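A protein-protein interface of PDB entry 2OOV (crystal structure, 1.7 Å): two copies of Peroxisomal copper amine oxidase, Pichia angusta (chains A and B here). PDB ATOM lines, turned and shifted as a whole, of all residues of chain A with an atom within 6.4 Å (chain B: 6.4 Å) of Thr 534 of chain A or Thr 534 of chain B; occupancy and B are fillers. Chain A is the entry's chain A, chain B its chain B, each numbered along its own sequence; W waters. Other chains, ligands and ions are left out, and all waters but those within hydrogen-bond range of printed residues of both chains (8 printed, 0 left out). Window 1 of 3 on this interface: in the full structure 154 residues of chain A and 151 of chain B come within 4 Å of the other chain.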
ATOM      1  N   TYR A 503     -10.791  19.769   8.072  1.00  0.00           N
ATOM      2  CA  TYR A 503      -9.394  19.600   8.406  1.00  0.00           C
ATOM      3  C   TYR A 503      -8.905  20.893   9.072  1.00  0.00           C
ATOM      4  O   TYR A 503      -9.297  22.000   8.659  1.00  0.00           O
ATOM      5  CB  TYR A 503      -8.541  19.235   7.173  1.00  0.00           C
ATOM      6  CG  TYR A 503      -7.086  19.144   7.566  1.00  0.00           C
ATOM      7  CD1 TYR A 503      -6.661  18.150   8.457  1.00  0.00           C
ATOM      8  CD2 TYR A 503      -6.148  20.082   7.109  1.00  0.00           C
ATOM      9  CE1 TYR A 503      -5.337  18.076   8.873  1.00  0.00           C
ATOM     10  CE2 TYR A 503      -4.810  20.026   7.531  1.00  0.00           C
ATOM     11  CZ  TYR A 503      -4.417  19.011   8.405  1.00  0.00           C
ATOM     12  OH  TYR A 503      -3.112  18.921   8.834  1.00  0.00           O
ATOM     13  N   SER A 505      -5.246  22.611  10.227  1.00  0.00           N
ATOM     14  CA  SER A 505      -3.797  22.626  10.338  1.00  0.00           C
ATOM     15  C   SER A 505      -3.365  22.927  11.783  1.00  0.00           C
ATOM     16  O   SER A 505      -2.337  22.433  12.242  1.00  0.00           O
ATOM     17  CB  SER A 505      -3.188  23.658   9.367  1.00  0.00           C
ATOM     18  OG  SER A 505      -3.830  24.915   9.497  1.00  0.00           O
ATOM     19  N   ARG A 509      -5.381  17.868  12.480  1.00  0.00           N
ATOM     20  CA  ARG A 509      -6.562  17.026  12.691  1.00  0.00           C
ATOM     21  C   ARG A 509      -6.516  15.742  11.881  1.00  0.00           C
ATOM     22  O   ARG A 509      -6.160  15.756  10.697  1.00  0.00           O
ATOM     23  CB  ARG A 509      -7.844  17.779  12.350  1.00  0.00           C
ATOM     24  CG  ARG A 509      -9.113  16.945  12.470  1.00  0.00           C
ATOM     25  CD  ARG A 509     -10.304  17.865  12.446  1.00  0.00           C
ATOM     26  NE  ARG A 509     -10.465  18.557  13.721  1.00  0.00           N
ATOM     27  CZ  ARG A 509     -11.442  19.426  13.967  1.00  0.00           C
ATOM     28  NH1 ARG A 509     -12.307  19.743  13.000  1.00  0.00           N
ATOM     29  NH2 ARG A 509     -11.556  19.974  15.172  1.00  0.00           N
ATOM     30  N   VAL A 532      -5.894   9.857   7.596  1.00  0.00           N
ATOM     31  CA  VAL A 532      -4.808  10.837   7.552  1.00  0.00           C
ATOM     32  C   VAL A 532      -4.873  11.526   6.180  1.00  0.00           C
ATOM     33  O   VAL A 532      -4.597  10.911   5.144  1.00  0.00           O
ATOM     34  CB  VAL A 532      -3.439  10.153   7.795  1.00  0.00           C
ATOM     35  CG1 VAL A 532      -2.297  11.151   7.689  1.00  0.00           C
ATOM     36  CG2 VAL A 532      -3.426   9.469   9.198  1.00  0.00           C
ATOM     37  N   SER A 533      -5.285  12.787   6.187  1.00  0.00           N
ATOM     38  CA  SER A 533      -5.666  13.470   4.953  1.00  0.00           C
ATOM     39  C   SER A 533      -5.536  14.969   5.157  1.00  0.00           C
ATOM     40  O   SER A 533      -6.214  15.543   6.011  1.00  0.00           O
ATOM     41  CB  SER A 533      -7.116  13.113   4.612  1.00  0.00           C
ATOM     42  OG  SER A 533      -7.510  13.677   3.375  1.00  0.00           O
ATOM     43  N   THR A 534      -4.658  15.600   4.385  1.00  0.00           N
ATOM     44  CA  THR A 534      -4.410  17.024   4.568  1.00  0.00           C
ATOM     45  C   THR A 534      -4.713  17.840   3.319  1.00  0.00           C
ATOM     46  O   THR A 534      -4.725  19.074   3.378  1.00  0.00           O
ATOM     47  CB  THR A 534      -2.956  17.310   5.017  1.00  0.00           C
ATOM     48  OG1 THR A 534      -2.036  16.951   3.965  1.00  0.00           O
ATOM     49  CG2 THR A 534      -2.622  16.532   6.310  1.00  0.00           C
ATOM     50  N   GLN A 535      -4.941  17.166   2.191  1.00  0.00           N
ATOM     51  CA  GLN A 535      -5.334  17.894   0.982  1.00  0.00           C
ATOM     52  C   GLN A 535      -6.851  18.092   1.030  1.00  0.00           C
ATOM     53  O   GLN A 535      -7.617  17.403   0.356  1.00  0.00           O
ATOM     54  CB  GLN A 535      -4.828  17.177  -0.287  1.00  0.00           C
ATOM     55  CG  GLN A 535      -3.319  17.336  -0.456  1.00  0.00           C
ATOM     56  CD  GLN A 535      -2.788  16.522  -1.636  1.00  0.00           C
ATOM     57  OE1 GLN A 535      -2.572  15.314  -1.520  1.00  0.00           O
ATOM     58  NE2 GLN A 535      -2.603  17.187  -2.786  1.00  0.00           N
ATOM     59  N   CYS A 536      -7.260  19.018   1.898  1.00  0.00           N
ATOM     60  CA  CYS A 536      -8.677  19.207   2.262  1.00  0.00           C
ATOM     61  C   CYS A 536      -9.060  20.679   2.129  1.00  0.00           C
ATOM     62  O   CYS A 536      -9.139  21.397   3.124  1.00  0.00           O
ATOM     63  CB  CYS A 536      -8.881  18.758   3.701  1.00  0.00           C
ATOM     64  SG  CYS A 536      -8.564  16.991   3.901  1.00  0.00           S
ATOM     65  N   PRO A 537      -9.304  21.134   0.893  1.00  0.00           N
ATOM     66  CA  PRO A 537      -9.566  22.562   0.666  1.00  0.00           C
ATOM     67  C   PRO A 537     -10.916  22.983   1.229  1.00  0.00           C
ATOM     68  O   PRO A 537     -11.877  22.208   1.146  1.00  0.00           O
ATOM     69  CB  PRO A 537      -9.617  22.678  -0.874  1.00  0.00           C
ATOM     70  CG  PRO A 537      -8.962  21.435  -1.395  1.00  0.00           C
ATOM     71  CD  PRO A 537      -9.323  20.365  -0.361  1.00  0.00           C
ATOM     72  N   HIS A 606     -15.938  11.814   3.012  1.00  0.00           N
ATOM     73  CA  HIS A 606     -14.803  12.685   3.202  1.00  0.00           C
ATOM     74  C   HIS A 606     -14.577  13.509   1.949  1.00  0.00           C
ATOM     75  O   HIS A 606     -14.465  12.958   0.844  1.00  0.00           O
ATOM     76  CB  HIS A 606     -13.553  11.849   3.521  1.00  0.00           C
ATOM     77  CG  HIS A 606     -12.287  12.640   3.613  1.00  0.00           C
ATOM     78  ND1 HIS A 606     -12.148  13.751   4.414  1.00  0.00           N
ATOM     79  CD2 HIS A 606     -11.078  12.441   3.031  1.00  0.00           C
ATOM     80  CE1 HIS A 606     -10.915  14.221   4.302  1.00  0.00           C
ATOM     81  NE2 HIS A 606     -10.245  13.443   3.468  1.00  0.00           N
ATOM     82  N   GLY A 609      -9.248  17.155  -1.990  1.00  0.00           N
ATOM     83  CA  GLY A 609      -8.913  17.589  -3.354  1.00  0.00           C
ATOM     84  C   GLY A 609      -7.896  18.720  -3.347  1.00  0.00           C
ATOM     85  O   GLY A 609      -7.082  18.846  -2.414  1.00  0.00           O
ATOM     86  N   THR A 628      -3.493  12.617  -2.318  1.00  0.00           N
ATOM     87  CA  THR A 628      -3.519  11.347  -1.584  1.00  0.00           C
ATOM     88  C   THR A 628      -4.206  11.486  -0.247  1.00  0.00           C
ATOM     89  O   THR A 628      -4.226  12.573   0.334  1.00  0.00           O
ATOM     90  CB  THR A 628      -2.075  10.740  -1.362  1.00  0.00           C
ATOM     91  OG1 THR A 628      -2.175   9.409  -0.823  1.00  0.00           O
ATOM     92  CG2 THR A 628      -1.206  11.622  -0.411  1.00  0.00           C
ATOM     93  N   LEU A 629      -4.780  10.377   0.215  1.00  0.00           N
ATOM     94  CA  LEU A 629      -5.196  10.238   1.603  1.00  0.00           C
ATOM     95  C   LEU A 629      -4.914   8.819   1.993  1.00  0.00           C
ATOM     96  O   LEU A 629      -4.769   7.952   1.129  1.00  0.00           O
ATOM     97  CB  LEU A 629      -6.684  10.571   1.812  1.00  0.00           C
ATOM     98  CG  LEU A 629      -7.944   9.810   1.340  1.00  0.00           C
ATOM     99  CD1 LEU A 629      -8.531  10.342   0.052  1.00  0.00           C
ATOM    100  CD2 LEU A 629      -7.954   8.259   1.398  1.00  0.00           C
ATOM    101  N   TYR B 503       1.684  27.331   7.970  1.00  0.00           N
ATOM    102  CA  TYR B 503       0.749  26.712   7.056  1.00  0.00           C
ATOM    103  C   TYR B 503      -0.665  26.991   7.565  1.00  0.00           C
ATOM    104  O   TYR B 503      -0.896  26.935   8.777  1.00  0.00           O
ATOM    105  CB  TYR B 503       0.983  25.188   6.938  1.00  0.00           C
ATOM    106  CG  TYR B 503      -0.037  24.580   6.009  1.00  0.00           C
ATOM    107  CD1 TYR B 503      -0.096  24.981   4.661  1.00  0.00           C
ATOM    108  CD2 TYR B 503      -1.006  23.691   6.476  1.00  0.00           C
ATOM    109  CE1 TYR B 503      -1.066  24.474   3.795  1.00  0.00           C
ATOM    110  CE2 TYR B 503      -2.001  23.187   5.611  1.00  0.00           C
ATOM    111  CZ  TYR B 503      -2.010  23.587   4.277  1.00  0.00           C
ATOM    112  OH  TYR B 503      -2.945  23.087   3.422  1.00  0.00           O
ATOM    113  N   SER B 505      -4.577  25.673   6.757  1.00  0.00           N
ATOM    114  CA  SER B 505      -5.514  24.863   6.007  1.00  0.00           C
ATOM    115  C   SER B 505      -6.667  25.719   5.461  1.00  0.00           C
ATOM    116  O   SER B 505      -7.204  25.417   4.387  1.00  0.00           O
ATOM    117  CB  SER B 505      -6.048  23.707   6.874  1.00  0.00           C
ATOM    118  OG  SER B 505      -6.542  24.170   8.119  1.00  0.00           O
ATOM    119  N   ARG B 509      -2.576  27.367   2.166  1.00  0.00           N
ATOM    120  CA  ARG B 509      -1.405  28.214   1.971  1.00  0.00           C
ATOM    121  C   ARG B 509      -0.241  27.500   1.273  1.00  0.00           C
ATOM    122  O   ARG B 509       0.101  26.372   1.620  1.00  0.00           O
ATOM    123  CB  ARG B 509      -0.914  28.771   3.313  1.00  0.00           C
ATOM    124  CG  ARG B 509       0.352  29.602   3.188  1.00  0.00           C
ATOM    125  CD  ARG B 509       0.558  30.375   4.471  1.00  0.00           C
ATOM    126  NE  ARG B 509      -0.371  31.499   4.551  1.00  0.00           N
ATOM    127  CZ  ARG B 509      -0.459  32.308   5.600  1.00  0.00           C
ATOM    128  NH1 ARG B 509       0.305  32.091   6.672  1.00  0.00           N
ATOM    129  NH2 ARG B 509      -1.300  33.337   5.578  1.00  0.00           N
ATOM    130  N   VAL B 532       5.040  23.583  -1.812  1.00  0.00           N
ATOM    131  CA  VAL B 532       3.770  22.915  -1.561  1.00  0.00           C
ATOM    132  C   VAL B 532       4.016  21.915  -0.432  1.00  0.00           C
ATOM    133  O   VAL B 532       4.700  20.904  -0.607  1.00  0.00           O
ATOM    134  CB  VAL B 532       3.249  22.234  -2.853  1.00  0.00           C
ATOM    135  CG1 VAL B 532       1.961  21.450  -2.598  1.00  0.00           C
ATOM    136  CG2 VAL B 532       3.049  23.307  -3.978  1.00  0.00           C
ATOM    137  N   SER B 533       3.511  22.238   0.748  1.00  0.00           N
ATOM    138  CA  SER B 533       3.886  21.501   1.943  1.00  0.00           C
ATOM    139  C   SER B 533       2.762  21.606   2.960  1.00  0.00           C
ATOM    140  O   SER B 533       2.419  22.702   3.393  1.00  0.00           O
ATOM    141  CB  SER B 533       5.173  22.109   2.505  1.00  0.00           C
ATOM    142  OG  SER B 533       5.653  21.415   3.639  1.00  0.00           O
ATOM    143  N   THR B 534       2.208  20.470   3.363  1.00  0.00           N
ATOM    144  CA  THR B 534       1.073  20.517   4.281  1.00  0.00           C
ATOM    145  C   THR B 534       1.341  19.759   5.582  1.00  0.00           C
ATOM    146  O   THR B 534       0.545  19.852   6.524  1.00  0.00           O
ATOM    147  CB  THR B 534      -0.228  19.972   3.649  1.00  0.00           C
ATOM    148  OG1 THR B 534      -0.068  18.578   3.372  1.00  0.00           O
ATOM    149  CG2 THR B 534      -0.595  20.735   2.348  1.00  0.00           C
ATOM    150  N   GLN B 535       2.450  19.020   5.642  1.00  0.00           N
ATOM    151  CA  GLN B 535       2.795  18.343   6.900  1.00  0.00           C
ATOM    152  C   GLN B 535       3.597  19.320   7.749  1.00  0.00           C
ATOM    153  O   GLN B 535       4.818  19.244   7.830  1.00  0.00           O
ATOM    154  CB  GLN B 535       3.516  17.017   6.630  1.00  0.00           C
ATOM    155  CG  GLN B 535       2.553  15.943   6.096  1.00  0.00           C
ATOM    156  CD  GLN B 535       3.285  14.664   5.699  1.00  0.00           C
ATOM    157  OE1 GLN B 535       3.863  14.580   4.614  1.00  0.00           O
ATOM    158  NE2 GLN B 535       3.297  13.678   6.607  1.00  0.00           N
ATOM    159  N   CYS B 536       2.875  20.286   8.326  1.00  0.00           N
ATOM    160  CA  CYS B 536       3.461  21.467   8.981  1.00  0.00           C
ATOM    161  C   CYS B 536       2.856  21.638  10.365  1.00  0.00           C
ATOM    162  O   CYS B 536       1.966  22.465  10.561  1.00  0.00           O
ATOM    163  CB  CYS B 536       3.196  22.711   8.143  1.00  0.00           C
ATOM    164  SG  CYS B 536       3.971  22.584   6.507  1.00  0.00           S
ATOM    165  N   PRO B 537       3.308  20.817  11.333  1.00  0.00           N
ATOM    166  CA  PRO B 537       2.665  20.887  12.658  1.00  0.00           C
ATOM    167  C   PRO B 537       3.002  22.190  13.388  1.00  0.00           C
ATOM    168  O   PRO B 537       4.142  22.671  13.304  1.00  0.00           O
ATOM    169  CB  PRO B 537       3.290  19.704  13.431  1.00  0.00           C
ATOM    170  CG  PRO B 537       3.951  18.824  12.380  1.00  0.00           C
ATOM    171  CD  PRO B 537       4.373  19.804  11.280  1.00  0.00           C
ATOM    172  N   HIS B 606      12.241  26.317   6.308  1.00  0.00           N
ATOM    173  CA  HIS B 606      10.896  25.782   6.380  1.00  0.00           C
ATOM    174  C   HIS B 606      10.829  24.697   7.430  1.00  0.00           C
ATOM    175  O   HIS B 606      11.622  23.757   7.393  1.00  0.00           O
ATOM    176  CB  HIS B 606      10.513  25.198   5.013  1.00  0.00           C
ATOM    177  CG  HIS B 606       9.181  24.514   4.992  1.00  0.00           C
ATOM    178  ND1 HIS B 606       8.023  25.121   5.420  1.00  0.00           N
ATOM    179  CD2 HIS B 606       8.822  23.284   4.550  1.00  0.00           C
ATOM    180  CE1 HIS B 606       7.005  24.288   5.259  1.00  0.00           C
ATOM    181  NE2 HIS B 606       7.463  23.171   4.726  1.00  0.00           N
ATOM    182  N   GLY B 609       7.132  18.416   9.372  1.00  0.00           N
ATOM    183  CA  GLY B 609       7.267  17.158  10.116  1.00  0.00           C
ATOM    184  C   GLY B 609       5.915  16.594  10.523  1.00  0.00           C
ATOM    185  O   GLY B 609       4.891  16.852   9.868  1.00  0.00           O
ATOM    186  N   THR B 628       6.523  14.423   3.322  1.00  0.00           N
ATOM    187  CA  THR B 628       6.934  14.979   2.025  1.00  0.00           C
ATOM    188  C   THR B 628       6.630  16.464   1.887  1.00  0.00           C
ATOM    189  O   THR B 628       5.697  16.978   2.516  1.00  0.00           O
ATOM    190  CB  THR B 628       6.278  14.203   0.813  1.00  0.00           C
ATOM    191  OG1 THR B 628       6.909  14.594  -0.414  1.00  0.00           O
ATOM    192  CG2 THR B 628       4.734  14.450   0.711  1.00  0.00           C
ATOM    193  N   LEU B 629       7.425  17.132   1.052  1.00  0.00           N
ATOM    194  CA  LEU B 629       7.181  18.504   0.621  1.00  0.00           C
ATOM    195  C   LEU B 629       7.690  18.582  -0.797  1.00  0.00           C
ATOM    196  O   LEU B 629       8.544  17.779  -1.199  1.00  0.00           O
ATOM    197  CB  LEU B 629       7.929  19.518   1.501  1.00  0.00           C
ATOM    198  CG  LEU B 629       9.458  19.381   1.616  1.00  0.00           C
ATOM    199  CD1 LEU B 629      10.203  20.206   0.543  1.00  0.00           C
ATOM    200  CD2 LEU B 629       9.915  19.795   3.002  1.00  0.00           C
HETATM  201  O   HOH W   1      -6.408  25.282  11.423  1.00  0.00           O
HETATM  202  O   HOH W   2      -9.096  24.826   7.996  1.00  0.00           O
HETATM  203  O   HOH W   3      -1.445  20.850   8.131  1.00  0.00           O
HETATM  204  O   HOH W   4      -6.071  27.418   8.893  1.00  0.00           O
HETATM  205  O   HOH W   5      -6.849  23.050   3.204  1.00  0.00           O
HETATM  206  O   HOH W   6      -0.556  21.170  10.693  1.00  0.00           O
HETATM  207  O   HOH W   7      -4.784  21.579   4.469  1.00  0.00           O
HETATM  208  O   HOH W   8      -2.431  26.349  11.190  1.00  0.00           O
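Of the 13 printed residues of chain A, 3 touch a printed residue of chain B.
Hydrophobic or aromatic side chains of chain B that line the printed part of chain A: Tyr 503.
Among the printed residues, no Asp or Glu carboxylate lies within 4 Å of a Lys or Arg side-chain nitrogen of the other chain.
Tyr 503 of chain A touches Ser 505 of chain B, and with the chains exchanged Ser 505 of chain A touches Tyr 503 of chain B.
Ser 505 of chain A touches its own counterpart, Ser 505 of chain B.
Thr 534 of chain A touches its own counterpart, Thr 534 of chain B.
13 positions are printed for both chains.
Of the 4 pairs that touch across the chains among the printed residues, 4 have their exchanged pair printed and touching as well.
Among the printed residues, merely in contact across the chains: Tyr 503 of chain A with Ser 505 of chain B (3.5 Å) and Ser 505 of chain A with Tyr 503 of chain B (3.6 Å).
OG1 of Thr 534 of chain B sits at hydrogen-bond distance from OG1 of Thr 534 of chain A (2.6 Å).
The backbone NH (N) of Ser 505 of chain A is in hydrogen-bond range of the side-chain hydroxyl (OG) of Ser 505 of chain B (2.9 Å).
Water W7 bridges OH of Tyr 503 of chain B (2.6 Å) and O of Thr 534 of chain A (2.7 Å).
Water W8 bridges the side-chain hydroxyl (OG) of Ser 505 of chain A (2.6 Å) and the backbone carbonyl oxygen (O) of Tyr 503 of chain B (2.9 Å).
Water W5 bridges O of Ser 505 of chain B (2.7 Å) and O of Cys 536 of chain A (2.8 Å).
Water W6 bridges the backbone carbonyl oxygen of Ser 505 of chain A and the backbone carbonyl oxygen of Cys 536 of chain B.
Water W4 lies within hydrogen-bond range of the backbone NH of Ser 505 of chain B (3.1 Å) and the side-chain hydroxyl of Ser 505 of chain A (3.4 Å).
Water W1 bridges the backbone NH (N) of Ser 505 of chain A and the side-chain hydroxyl (OG) of Ser 505 of chain B.
Of the printed residues of chain B, Ser 505 of chain A touches Tyr 503 (3.6 Å) and Ser 505 (2.9 Å).
Printed residues of chain A within 4 Å of Ser 505 of chain B: Tyr 503 (3.5 Å) and Ser 505 (2.9 Å).
Of the printed residues of chain B, Tyr 503 of chain A touches Ser 505 (3.5 Å).
Of the printed residues of chain A, Tyr 503 of chain B touches Ser 505 (3.6 Å).
Gln 535 of chain A touches none of the printed residues of chain B.
The nearest residue of chain B that does not touch Thr 534 of chain A is Tyr 503 of chain B (4.4 Å).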
